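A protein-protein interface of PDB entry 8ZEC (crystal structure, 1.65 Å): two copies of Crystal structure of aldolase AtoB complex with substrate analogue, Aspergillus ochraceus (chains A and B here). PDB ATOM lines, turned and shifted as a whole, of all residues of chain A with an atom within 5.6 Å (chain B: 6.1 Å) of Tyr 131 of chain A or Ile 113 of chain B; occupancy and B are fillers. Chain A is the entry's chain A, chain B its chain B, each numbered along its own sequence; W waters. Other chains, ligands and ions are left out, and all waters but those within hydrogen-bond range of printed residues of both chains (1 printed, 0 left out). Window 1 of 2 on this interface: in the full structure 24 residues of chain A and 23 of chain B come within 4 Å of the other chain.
The side-chain hydroxyl (OH) of Tyr 131 of chain B lies within hydrogen-bond range of the backbone carbonyl oxygen (O) of Glu 111 of chain A. The side-chain hydroxyl (OH) of Tyr 131 of chain A is in hydrogen-bond range of the backbone carbonyl oxygen (O) of Glu 111 of chain B (2.6 Å). OH of Tyr 131 of chain A is in hydrogen-bond range of N of Asp 133 of chain B, 3.1 Å away. N of Asp 133 of chain A is in hydrogen-bond range of OH of Tyr 131 of chain B (3.1 Å). The side-chain carboxylate (OD1) of Asp 133 of chain A lies within hydrogen-bond range of the side-chain hydroxyl (OG1) of Thr 134 of chain B (2.7 Å). The side-chain hydroxyl of Thr 134 of chain A is in hydrogen-bond range of the side-chain carboxylate of Asp 133 of chain B (2.7 Å). The side-chain hydroxyl of Thr 134 of chain B is in hydrogen-bond range of the backbone NH of Thr 134 of chain A (3.0 Å).
N of Leu 44 of chain A sits at hydrogen-bond distance from O of Glu 130 of chain A (2.8 Å). The backbone NH of Val 132 of chain A lies within hydrogen-bond range of the backbone carbonyl oxygen of Leu 44 of chain A (3.0 Å). The backbone carbonyl oxygen (O) of Ile 113 of chain A is in hydrogen-bond range of the backbone NH (N) of Tyr 131 of chain A (2.8 Å). The side-chain carboxylate (OE2) of Glu 111 of chain B sits at hydrogen-bond distance from a ring nitrogen (NE2) of His 96 of chain B, 2.7 Å away. The backbone carbonyl oxygen (O) of Met 97 of chain B is in hydrogen-bond range of the backbone NH (N) of Phe 112 of chain B. O of Ile 113 of chain B sits at hydrogen-bond distance from N of Tyr 131 of chain B, 2.8 Å away.
Among the printed residues, merely in contact across the chains: Val 132 of chain A with Tyr 131 of chain B (3.3 Å), Tyr 131 of chain A with Val 132 of chain B (3.4 Å), Tyr 131 of chain A with Tyr 131 of chain B (3.4 Å), Pro 45 of chain A with Glu 111 of chain B (3.4 Å), Ile 113 of chain A with Tyr 131 of chain B (3.6 Å), Leu 44 of chain A with His 96 of chain B (3.6 Å), Tyr 131 of chain A with Ile 113 of chain B (3.7 Å), Pro 45 of chain A with Asp 133 of chain B (3.7 Å), Tyr 131 of chain A with Phe 112 of chain B (3.8 Å) and Phe 112 of chain A with Tyr 131 of chain B (3.99 Å).
Of the printed residues of chain B, Pro 45 of chain A touches Glu 111 and Asp 133. Of the printed residues of chain B, Tyr 131 of chain A touches Glu 111, Phe 112, Ile 113, Tyr 131, Val 132 and Asp 133. Ile 113 of chain B touches just one residue of chain A: Tyr 131. Of the printed residues of chain A, Asp 133 of chain B touches Pro 45 (3.7 Å), Tyr 131 (3.1 Å) and Thr 134 (2.7 Å). The nearest residue of chain B that does not touch Tyr 131 of chain A is His 96 of chain B (5.0 Å).
Hydrophobic or aromatic side chains of chain A within 4 Å of the printed part of chain B: Leu 44, Pro 45, Ile 113 and Tyr 131. Hydrophobic or aromatic side chains of chain B within 4 Å of the printed part of chain A: His 96, Ile 113 and Tyr 131.
Tyr 131 of chain A touches its own counterpart, Tyr 131 of chain B. Tyr 131 of chain A touches Val 132 of chain B, and with the chains exchanged Val 132 of chain A touches Tyr 131 of chain B. Tyr 131 of chain A touches Asp 133 of chain B, and with the chains exchanged Asp 133 of chain A touches Tyr 131 of chain B. Asp 133 of chain A touches Thr 134 of chain B, and with the chains exchanged Thr 134 of chain A touches Asp 133 of chain B. Of the 17 pairs that touch across the chains among the printed residues, 14 have their exchanged pair printed and touching as well.
Water W1 lies within hydrogen-bond range of the backbone carbonyl oxygen (O) of Val 132 of chain A (2.7 Å), the backbone carbonyl oxygen (O) of Val 132 of chain B (2.8 Å), the backbone NH (N) of Thr 134 of chain A (3.0 Å) and the backbone NH (N) of Thr 134 of chain B (3.0 Å).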
ATOM      1  N   LYS A  42     -12.937  15.287 -15.878  1.00  0.00           N
ATOM      2  CA  LYS A  42     -12.957  14.193 -14.928  1.00  0.00           C
ATOM      3  C   LYS A  42     -11.609  14.150 -14.230  1.00  0.00           C
ATOM      4  O   LYS A  42     -10.568  14.275 -14.876  1.00  0.00           O
ATOM      5  CB  LYS A  42     -13.195  12.840 -15.591  1.00  0.00           C
ATOM      6  CG  LYS A  42     -14.446  12.741 -16.439  1.00  0.00           C
ATOM      7  CD  LYS A  42     -14.797  11.334 -16.817  1.00  0.00           C
ATOM      8  CE  LYS A  42     -16.193  11.193 -17.398  1.00  0.00           C
ATOM      9  NZ  LYS A  42     -16.665   9.802 -17.286  1.00  0.00           N
ATOM     10  N   LEU A  44      -9.212  12.025 -11.853  1.00  0.00           N
ATOM     11  CA  LEU A  44      -8.849  10.661 -11.504  1.00  0.00           C
ATOM     12  C   LEU A  44      -7.745  10.721 -10.458  1.00  0.00           C
ATOM     13  O   LEU A  44      -6.924  11.647 -10.460  1.00  0.00           O
ATOM     14  CB  LEU A  44      -8.345   9.920 -12.751  1.00  0.00           C
ATOM     15  CG  LEU A  44      -9.133  10.045 -14.047  1.00  0.00           C
ATOM     16  CD1 LEU A  44      -8.543   9.128 -15.092  1.00  0.00           C
ATOM     17  CD2 LEU A  44     -10.575   9.804 -13.851  1.00  0.00           C
ATOM     18  N   PRO A  45      -7.624   9.767  -9.522  1.00  0.00           N
ATOM     19  CA  PRO A  45      -8.550   8.653  -9.338  1.00  0.00           C
ATOM     20  C   PRO A  45      -9.802   9.086  -8.562  1.00  0.00           C
ATOM     21  O   PRO A  45      -9.807  10.141  -7.898  1.00  0.00           O
ATOM     22  CB  PRO A  45      -7.697   7.676  -8.533  1.00  0.00           C
ATOM     23  CG  PRO A  45      -6.909   8.605  -7.652  1.00  0.00           C
ATOM     24  CD  PRO A  45      -6.564   9.798  -8.509  1.00  0.00           C
ATOM     25  N   GLU A 111       2.836  16.531 -11.532  1.00  0.00           N
ATOM     26  CA  GLU A 111       2.924  15.614 -12.661  1.00  0.00           C
ATOM     27  C   GLU A 111       1.582  14.889 -12.823  1.00  0.00           C
ATOM     28  O   GLU A 111       0.924  14.589 -11.813  1.00  0.00           O
ATOM     29  CB  GLU A 111       4.097  14.671 -12.406  1.00  0.00           C
ATOM     30  CG  GLU A 111       4.193  13.543 -13.366  1.00  0.00           C
ATOM     31  CD  GLU A 111       5.358  12.609 -13.070  1.00  0.00           C
ATOM     32  OE1 GLU A 111       6.182  12.909 -12.162  1.00  0.00           O
ATOM     33  OE2 GLU A 111       5.426  11.571 -13.749  1.00  0.00           O
ATOM     34  N   PHE A 112       1.188  14.600 -14.086  1.00  0.00           N
ATOM     35  CA  PHE A 112      -0.186  14.249 -14.428  1.00  0.00           C
ATOM     36  C   PHE A 112      -0.161  13.309 -15.617  1.00  0.00           C
ATOM     37  O   PHE A 112       0.801  13.389 -16.415  1.00  0.00           O
ATOM     38  CB  PHE A 112      -1.029  15.452 -14.905  1.00  0.00           C
ATOM     39  CG  PHE A 112      -1.169  16.549 -13.883  1.00  0.00           C
ATOM     40  CD1 PHE A 112      -0.227  17.552 -13.740  1.00  0.00           C
ATOM     41  CD2 PHE A 112      -2.267  16.542 -13.071  1.00  0.00           C
ATOM     42  CE1 PHE A 112      -0.378  18.525 -12.764  1.00  0.00           C
ATOM     43  CE2 PHE A 112      -2.438  17.533 -12.120  1.00  0.00           C
ATOM     44  CZ  PHE A 112      -1.490  18.530 -11.973  1.00  0.00           C
ATOM     45  N   ILE A 113      -1.194  12.465 -15.716  1.00  0.00           N
ATOM     46  CA  ILE A 113      -1.614  11.978 -17.036  1.00  0.00           C
ATOM     47  C   ILE A 113      -2.861  12.739 -17.455  1.00  0.00           C
ATOM     48  O   ILE A 113      -3.817  12.838 -16.670  1.00  0.00           O
ATOM     49  CB  ILE A 113      -1.873  10.462 -17.037  1.00  0.00           C
ATOM     50  CG1 ILE A 113      -0.685   9.654 -16.528  1.00  0.00           C
ATOM     51  CG2 ILE A 113      -2.372  10.009 -18.358  1.00  0.00           C
ATOM     52  CD1 ILE A 113       0.467   9.753 -17.424  1.00  0.00           C
ATOM     53  N   PHE A 114      -2.901  13.204 -18.699  1.00  0.00           N
ATOM     54  CA  PHE A 114      -4.157  13.734 -19.250  1.00  0.00           C
ATOM     55  C   PHE A 114      -4.609  12.848 -20.429  1.00  0.00           C
ATOM     56  O   PHE A 114      -3.782  12.435 -21.308  1.00  0.00           O
ATOM     57  CB  PHE A 114      -3.935  15.124 -19.823  1.00  0.00           C
ATOM     58  CG  PHE A 114      -3.871  16.262 -18.831  1.00  0.00           C
ATOM     59  CD1 PHE A 114      -2.763  16.501 -18.024  1.00  0.00           C
ATOM     60  CD2 PHE A 114      -5.024  17.009 -18.613  1.00  0.00           C
ATOM     61  CE1 PHE A 114      -2.791  17.521 -17.073  1.00  0.00           C
ATOM     62  CE2 PHE A 114      -5.069  17.937 -17.598  1.00  0.00           C
ATOM     63  CZ  PHE A 114      -3.954  18.250 -16.870  1.00  0.00           C
ATOM     64  N   ILE A 115      -5.889  12.547 -20.452  1.00  0.00           N
ATOM     65  CA  ILE A 115      -6.538  11.835 -21.563  1.00  0.00           C
ATOM     66  C   ILE A 115      -7.612  12.773 -22.104  1.00  0.00           C
ATOM     67  O   ILE A 115      -8.532  13.150 -21.370  1.00  0.00           O
ATOM     68  CB  ILE A 115      -7.198  10.512 -21.130  1.00  0.00           C
ATOM     69  CG1 ILE A 115      -6.263   9.527 -20.425  1.00  0.00           C
ATOM     70  CG2 ILE A 115      -7.823   9.862 -22.348  1.00  0.00           C
ATOM     71  CD1 ILE A 115      -7.005   8.370 -19.764  1.00  0.00           C
ATOM     72  N   ALA A 129      -9.801  14.051 -18.991  1.00  0.00           N
ATOM     73  CA  ALA A 129      -9.658  13.279 -17.784  1.00  0.00           C
ATOM     74  C   ALA A 129      -8.207  13.470 -17.363  1.00  0.00           C
ATOM     75  O   ALA A 129      -7.297  13.337 -18.181  1.00  0.00           O
ATOM     76  CB  ALA A 129      -9.983  11.828 -18.003  1.00  0.00           C
ATOM     77  N   GLU A 130      -8.006  13.851 -16.095  1.00  0.00           N
ATOM     78  CA  GLU A 130      -6.651  14.073 -15.602  1.00  0.00           C
ATOM     79  C   GLU A 130      -6.445  13.222 -14.365  1.00  0.00           C
ATOM     80  O   GLU A 130      -7.211  13.290 -13.405  1.00  0.00           O
ATOM     81  CB  GLU A 130      -6.364  15.556 -15.330  1.00  0.00           C
ATOM     82  CG  GLU A 130      -7.098  16.159 -14.173  1.00  0.00           C
ATOM     83  CD  GLU A 130      -6.779  17.639 -14.033  1.00  0.00           C
ATOM     84  OE1 GLU A 130      -5.569  18.013 -13.997  1.00  0.00           O
ATOM     85  OE2 GLU A 130      -7.734  18.411 -13.924  1.00  0.00           O
ATOM     86  N   TYR A 131      -5.388  12.392 -14.403  1.00  0.00           N
ATOM     87  CA  TYR A 131      -5.018  11.611 -13.236  1.00  0.00           C
ATOM     88  C   TYR A 131      -3.929  12.395 -12.515  1.00  0.00           C
ATOM     89  O   TYR A 131      -2.900  12.766 -13.096  1.00  0.00           O
ATOM     90  CB  TYR A 131      -4.605  10.212 -13.654  1.00  0.00           C
ATOM     91  CG  TYR A 131      -4.467   9.174 -12.546  1.00  0.00           C
ATOM     92  CD1 TYR A 131      -3.736   9.415 -11.401  1.00  0.00           C
ATOM     93  CD2 TYR A 131      -5.202   7.991 -12.556  1.00  0.00           C
ATOM     94  CE1 TYR A 131      -3.649   8.465 -10.383  1.00  0.00           C
ATOM     95  CE2 TYR A 131      -5.097   7.010 -11.574  1.00  0.00           C
ATOM     96  CZ  TYR A 131      -4.394   7.301 -10.418  1.00  0.00           C
ATOM     97  OH  TYR A 131      -4.321   6.405  -9.388  1.00  0.00           O
ATOM     98  N   VAL A 132      -4.209  12.722 -11.265  1.00  0.00           N
ATOM     99  CA  VAL A 132      -3.395  13.635 -10.489  1.00  0.00           C
ATOM    100  C   VAL A 132      -2.575  12.857  -9.429  1.00  0.00           C
ATOM    101  O   VAL A 132      -2.882  11.710  -9.077  1.00  0.00           O
ATOM    102  CB  VAL A 132      -4.299  14.683  -9.794  1.00  0.00           C
ATOM    103  CG1 VAL A 132      -5.261  15.413 -10.724  1.00  0.00           C
ATOM    104  CG2 VAL A 132      -5.035  14.035  -8.673  1.00  0.00           C
ATOM    105  N   ASP A 133      -1.629  13.572  -8.807  1.00  0.00           N
ATOM    106  CA  ASP A 133      -0.796  13.068  -7.723  1.00  0.00           C
ATOM    107  C   ASP A 133      -1.553  13.296  -6.414  1.00  0.00           C
ATOM    108  O   ASP A 133      -1.563  14.451  -5.920  1.00  0.00           O
ATOM    109  CB  ASP A 133       0.588  13.723  -7.828  1.00  0.00           C
ATOM    110  CG  ASP A 133       1.570  13.390  -6.709  1.00  0.00           C
ATOM    111  OD1 ASP A 133       1.161  12.749  -5.706  1.00  0.00           O
ATOM    112  OD2 ASP A 133       2.763  13.731  -6.860  1.00  0.00           O
ATOM    113  N   THR A 134      -2.180  12.235  -5.860  1.00  0.00           N
ATOM    114  CA  THR A 134      -3.236  12.462  -4.845  1.00  0.00           C
ATOM    115  C   THR A 134      -2.605  13.028  -3.565  1.00  0.00           C
ATOM    116  O   THR A 134      -3.122  13.938  -2.909  1.00  0.00           O
ATOM    117  CB  THR A 134      -4.083  11.197  -4.597  1.00  0.00           C
ATOM    118  OG1 THR A 134      -3.182  10.095  -4.404  1.00  0.00           O
ATOM    119  CG2 THR A 134      -4.999  10.861  -5.760  1.00  0.00           C
ATOM    120  N   VAL B  94      -2.893   2.502 -23.781  1.00  0.00           N
ATOM    121  CA  VAL B  94      -3.191   3.111 -22.500  1.00  0.00           C
ATOM    122  C   VAL B  94      -4.488   2.529 -21.997  1.00  0.00           C
ATOM    123  O   VAL B  94      -5.523   2.515 -22.693  1.00  0.00           O
ATOM    124  CB  VAL B  94      -3.246   4.641 -22.588  1.00  0.00           C
ATOM    125  CG1 VAL B  94      -3.504   5.306 -21.237  1.00  0.00           C
ATOM    126  CG2 VAL B  94      -2.023   5.239 -23.230  1.00  0.00           C
ATOM    127  N   PHE B  95      -4.421   2.106 -20.731  1.00  0.00           N
ATOM    128  CA  PHE B  95      -5.526   1.552 -19.994  1.00  0.00           C
ATOM    129  C   PHE B  95      -5.728   2.336 -18.714  1.00  0.00           C
ATOM    130  O   PHE B  95      -4.781   2.721 -18.034  1.00  0.00           O
ATOM    131  CB  PHE B  95      -5.330   0.100 -19.539  1.00  0.00           C
ATOM    132  CG  PHE B  95      -5.108  -0.905 -20.649  1.00  0.00           C
ATOM    133  CD1 PHE B  95      -6.133  -1.301 -21.477  1.00  0.00           C
ATOM    134  CD2 PHE B  95      -3.864  -1.453 -20.865  1.00  0.00           C
ATOM    135  CE1 PHE B  95      -5.951  -2.270 -22.445  1.00  0.00           C
ATOM    136  CE2 PHE B  95      -3.666  -2.404 -21.857  1.00  0.00           C
ATOM    137  CZ  PHE B  95      -4.712  -2.808 -22.655  1.00  0.00           C
ATOM    138  N   HIS B  96      -7.014   2.476 -18.367  1.00  0.00           N
ATOM    139  CA  HIS B  96      -7.435   3.003 -17.080  1.00  0.00           C
ATOM    140  C   HIS B  96      -7.988   1.816 -16.293  1.00  0.00           C
ATOM    141  O   HIS B  96      -9.015   1.235 -16.657  1.00  0.00           O
ATOM    142  CB  HIS B  96      -8.537   4.054 -17.320  1.00  0.00           C
ATOM    143  CG  HIS B  96      -9.053   4.773 -16.142  1.00  0.00           C
ATOM    144  ND1 HIS B  96     -10.222   5.519 -16.120  1.00  0.00           N
ATOM    145  CD2 HIS B  96      -8.524   4.853 -14.938  1.00  0.00           C
ATOM    146  CE1 HIS B  96     -10.384   6.002 -14.904  1.00  0.00           C
ATOM    147  NE2 HIS B  96      -9.358   5.655 -14.166  1.00  0.00           N
ATOM    148  N   MET B  97      -7.287   1.389 -15.252  1.00  0.00           N
ATOM    149  CA  MET B  97      -7.471   0.076 -14.634  1.00  0.00           C
ATOM    150  C   MET B  97      -7.733   0.149 -13.132  1.00  0.00           C
ATOM    151  O   MET B  97      -7.319   1.105 -12.459  1.00  0.00           O
ATOM    152  CB  MET B  97      -6.199  -0.733 -14.793  1.00  0.00           C
ATOM    153  CG  MET B  97      -5.800  -0.999 -16.194  1.00  0.00           C
ATOM    154  SD  MET B  97      -6.953  -2.092 -17.060  1.00  0.00           S
ATOM    155  CE  MET B  97      -6.927  -3.583 -16.089  1.00  0.00           C
ATOM    156  N   GLU B 111      -6.670   2.229  -8.205  1.00  0.00           N
ATOM    157  CA  GLU B 111      -6.935   2.756  -9.533  1.00  0.00           C
ATOM    158  C   GLU B 111      -5.649   3.287 -10.162  1.00  0.00           C
ATOM    159  O   GLU B 111      -4.823   3.877  -9.456  1.00  0.00           O
ATOM    160  CB  GLU B 111      -7.964   3.894  -9.461  1.00  0.00           C
ATOM    161  CG  GLU B 111      -8.410   4.450 -10.772  1.00  0.00           C
ATOM    162  CD  GLU B 111      -9.522   5.477 -10.671  1.00  0.00           C
ATOM    163  OE1 GLU B 111     -10.237   5.480  -9.643  1.00  0.00           O
ATOM    164  OE2 GLU B 111      -9.647   6.280 -11.582  1.00  0.00           O
ATOM    165  N   PHE B 112      -5.486   3.035 -11.467  1.00  0.00           N
ATOM    166  CA  PHE B 112      -4.272   3.320 -12.192  1.00  0.00           C
ATOM    167  C   PHE B 112      -4.500   3.795 -13.610  1.00  0.00           C
ATOM    168  O   PHE B 112      -5.551   3.532 -14.218  1.00  0.00           O
ATOM    169  CB  PHE B 112      -3.423   2.048 -12.326  1.00  0.00           C
ATOM    170  CG  PHE B 112      -3.127   1.318 -11.054  1.00  0.00           C
ATOM    171  CD1 PHE B 112      -4.042   0.450 -10.495  1.00  0.00           C
ATOM    172  CD2 PHE B 112      -1.921   1.508 -10.408  1.00  0.00           C
ATOM    173  CE1 PHE B 112      -3.739  -0.246  -9.335  1.00  0.00           C
ATOM    174  CE2 PHE B 112      -1.620   0.801  -9.254  1.00  0.00           C
ATOM    175  CZ  PHE B 112      -2.540  -0.040  -8.690  1.00  0.00           C
ATOM    176  N   ILE B 113      -3.448   4.403 -14.155  1.00  0.00           N
ATOM    177  CA  ILE B 113      -3.250   4.457 -15.591  1.00  0.00           C
ATOM    178  C   ILE B 113      -2.032   3.593 -15.911  1.00  0.00           C
ATOM    179  O   ILE B 113      -0.994   3.677 -15.240  1.00  0.00           O
ATOM    180  CB  ILE B 113      -2.997   5.857 -16.168  1.00  0.00           C
ATOM    181  CG1 ILE B 113      -4.095   6.845 -15.840  1.00  0.00           C
ATOM    182  CG2 ILE B 113      -2.790   5.798 -17.654  1.00  0.00           C
ATOM    183  CD1 ILE B 113      -5.352   6.481 -16.381  1.00  0.00           C
ATOM    184  N   PHE B 114      -2.178   2.750 -16.923  1.00  0.00           N
ATOM    185  CA  PHE B 114      -1.057   2.008 -17.491  1.00  0.00           C
ATOM    186  C   PHE B 114      -0.809   2.449 -18.921  1.00  0.00           C
ATOM    187  O   PHE B 114      -1.740   2.648 -19.706  1.00  0.00           O
ATOM    188  CB  PHE B 114      -1.382   0.516 -17.497  1.00  0.00           C
ATOM    189  CG  PHE B 114      -1.217  -0.184 -16.178  1.00  0.00           C
ATOM    190  CD1 PHE B 114      -2.223  -0.127 -15.212  1.00  0.00           C
ATOM    191  CD2 PHE B 114      -0.021  -0.770 -15.836  1.00  0.00           C
ATOM    192  CE1 PHE B 114      -2.093  -0.778 -13.998  1.00  0.00           C
ATOM    193  CE2 PHE B 114       0.142  -1.331 -14.569  1.00  0.00           C
ATOM    194  CZ  PHE B 114      -0.881  -1.352 -13.673  1.00  0.00           C
ATOM    195  N   ILE B 115       0.466   2.646 -19.234  1.00  0.00           N
ATOM    196  CA  ILE B 115       0.948   2.958 -20.571  1.00  0.00           C
ATOM    197  C   ILE B 115       1.912   1.852 -20.936  1.00  0.00           C
ATOM    198  O   ILE B 115       2.936   1.647 -20.286  1.00  0.00           O
ATOM    199  CB  ILE B 115       1.621   4.347 -20.675  1.00  0.00           C
ATOM    200  CG1 ILE B 115       0.656   5.458 -20.233  1.00  0.00           C
ATOM    201  CG2 ILE B 115       2.143   4.597 -22.071  1.00  0.00           C
ATOM    202  CD1 ILE B 115       1.189   6.830 -20.324  1.00  0.00           C
ATOM    203  N   ALA B 129       4.563   1.664 -17.997  1.00  0.00           N
ATOM    204  CA  ALA B 129       4.577   2.801 -17.110  1.00  0.00           C
ATOM    205  C   ALA B 129       3.237   2.841 -16.396  1.00  0.00           C
ATOM    206  O   ALA B 129       2.191   2.807 -17.049  1.00  0.00           O
ATOM    207  CB  ALA B 129       4.837   4.050 -17.915  1.00  0.00           C
ATOM    208  N   GLU B 130       3.254   2.928 -15.064  1.00  0.00           N
ATOM    209  CA  GLU B 130       2.003   2.901 -14.327  1.00  0.00           C
ATOM    210  C   GLU B 130       1.975   4.132 -13.418  1.00  0.00           C
ATOM    211  O   GLU B 130       2.924   4.397 -12.681  1.00  0.00           O
ATOM    212  CB  GLU B 130       1.815   1.645 -13.493  1.00  0.00           C
ATOM    213  CG  GLU B 130       2.818   1.371 -12.436  1.00  0.00           C
ATOM    214  CD  GLU B 130       2.526   0.022 -11.792  1.00  0.00           C
ATOM    215  OE1 GLU B 130       1.338  -0.306 -11.544  1.00  0.00           O
ATOM    216  OE2 GLU B 130       3.476  -0.672 -11.503  1.00  0.00           O
ATOM    217  N   TYR B 131       0.895   4.910 -13.544  1.00  0.00           N
ATOM    218  CA  TYR B 131       0.649   6.059 -12.685  1.00  0.00           C
ATOM    219  C   TYR B 131      -0.286   5.548 -11.590  1.00  0.00           C
ATOM    220  O   TYR B 131      -1.413   5.084 -11.906  1.00  0.00           O
ATOM    221  CB  TYR B 131       0.045   7.213 -13.531  1.00  0.00           C
ATOM    222  CG  TYR B 131       0.156   8.551 -12.808  1.00  0.00           C
ATOM    223  CD1 TYR B 131      -0.451   8.712 -11.578  1.00  0.00           C
ATOM    224  CD2 TYR B 131       0.869   9.629 -13.319  1.00  0.00           C
ATOM    225  CE1 TYR B 131      -0.402   9.923 -10.914  1.00  0.00           C
ATOM    226  CE2 TYR B 131       0.941  10.850 -12.657  1.00  0.00           C
ATOM    227  CZ  TYR B 131       0.354  10.972 -11.420  1.00  0.00           C
ATOM    228  OH  TYR B 131       0.361  12.182 -10.771  1.00  0.00           O
ATOM    229  N   VAL B 132       0.185   5.669 -10.344  1.00  0.00           N
ATOM    230  CA  VAL B 132      -0.442   5.106  -9.179  1.00  0.00           C
ATOM    231  C   VAL B 132      -1.124   6.214  -8.367  1.00  0.00           C
ATOM    232  O   VAL B 132      -0.822   7.384  -8.553  1.00  0.00           O
ATOM    233  CB  VAL B 132       0.566   4.334  -8.306  1.00  0.00           C
ATOM    234  CG1 VAL B 132       1.370   3.349  -9.166  1.00  0.00           C
ATOM    235  CG2 VAL B 132       1.496   5.239  -7.495  1.00  0.00           C
ATOM    236  N   ASP B 133      -1.987   5.772  -7.461  1.00  0.00           N
ATOM    237  CA  ASP B 133      -2.648   6.593  -6.455  1.00  0.00           C
ATOM    238  C   ASP B 133      -1.659   6.790  -5.303  1.00  0.00           C
ATOM    239  O   ASP B 133      -1.431   5.875  -4.507  1.00  0.00           O
ATOM    240  CB  ASP B 133      -3.939   5.889  -6.033  1.00  0.00           C
ATOM    241  CG  ASP B 133      -4.759   6.680  -5.044  1.00  0.00           C
ATOM    242  OD1 ASP B 133      -4.147   7.584  -4.347  1.00  0.00           O
ATOM    243  OD2 ASP B 133      -5.938   6.330  -4.908  1.00  0.00           O
ATOM    244  N   THR B 134      -1.000   7.944  -5.258  1.00  0.00           N
ATOM    245  CA  THR B 134       0.170   8.112  -4.374  1.00  0.00           C
ATOM    246  C   THR B 134      -0.270   8.059  -2.900  1.00  0.00           C
ATOM    247  O   THR B 134       0.344   7.378  -2.080  1.00  0.00           O
ATOM    248  CB  THR B 134       0.961   9.392  -4.725  1.00  0.00           C
ATOM    249  OG1 THR B 134       0.081  10.515  -4.760  1.00  0.00           O
ATOM    250  CG2 THR B 134       1.651   9.340  -6.066  1.00  0.00           C
HETATM  251  O   HOH W   1      -1.767   9.823  -7.532  1.00  0.00           O
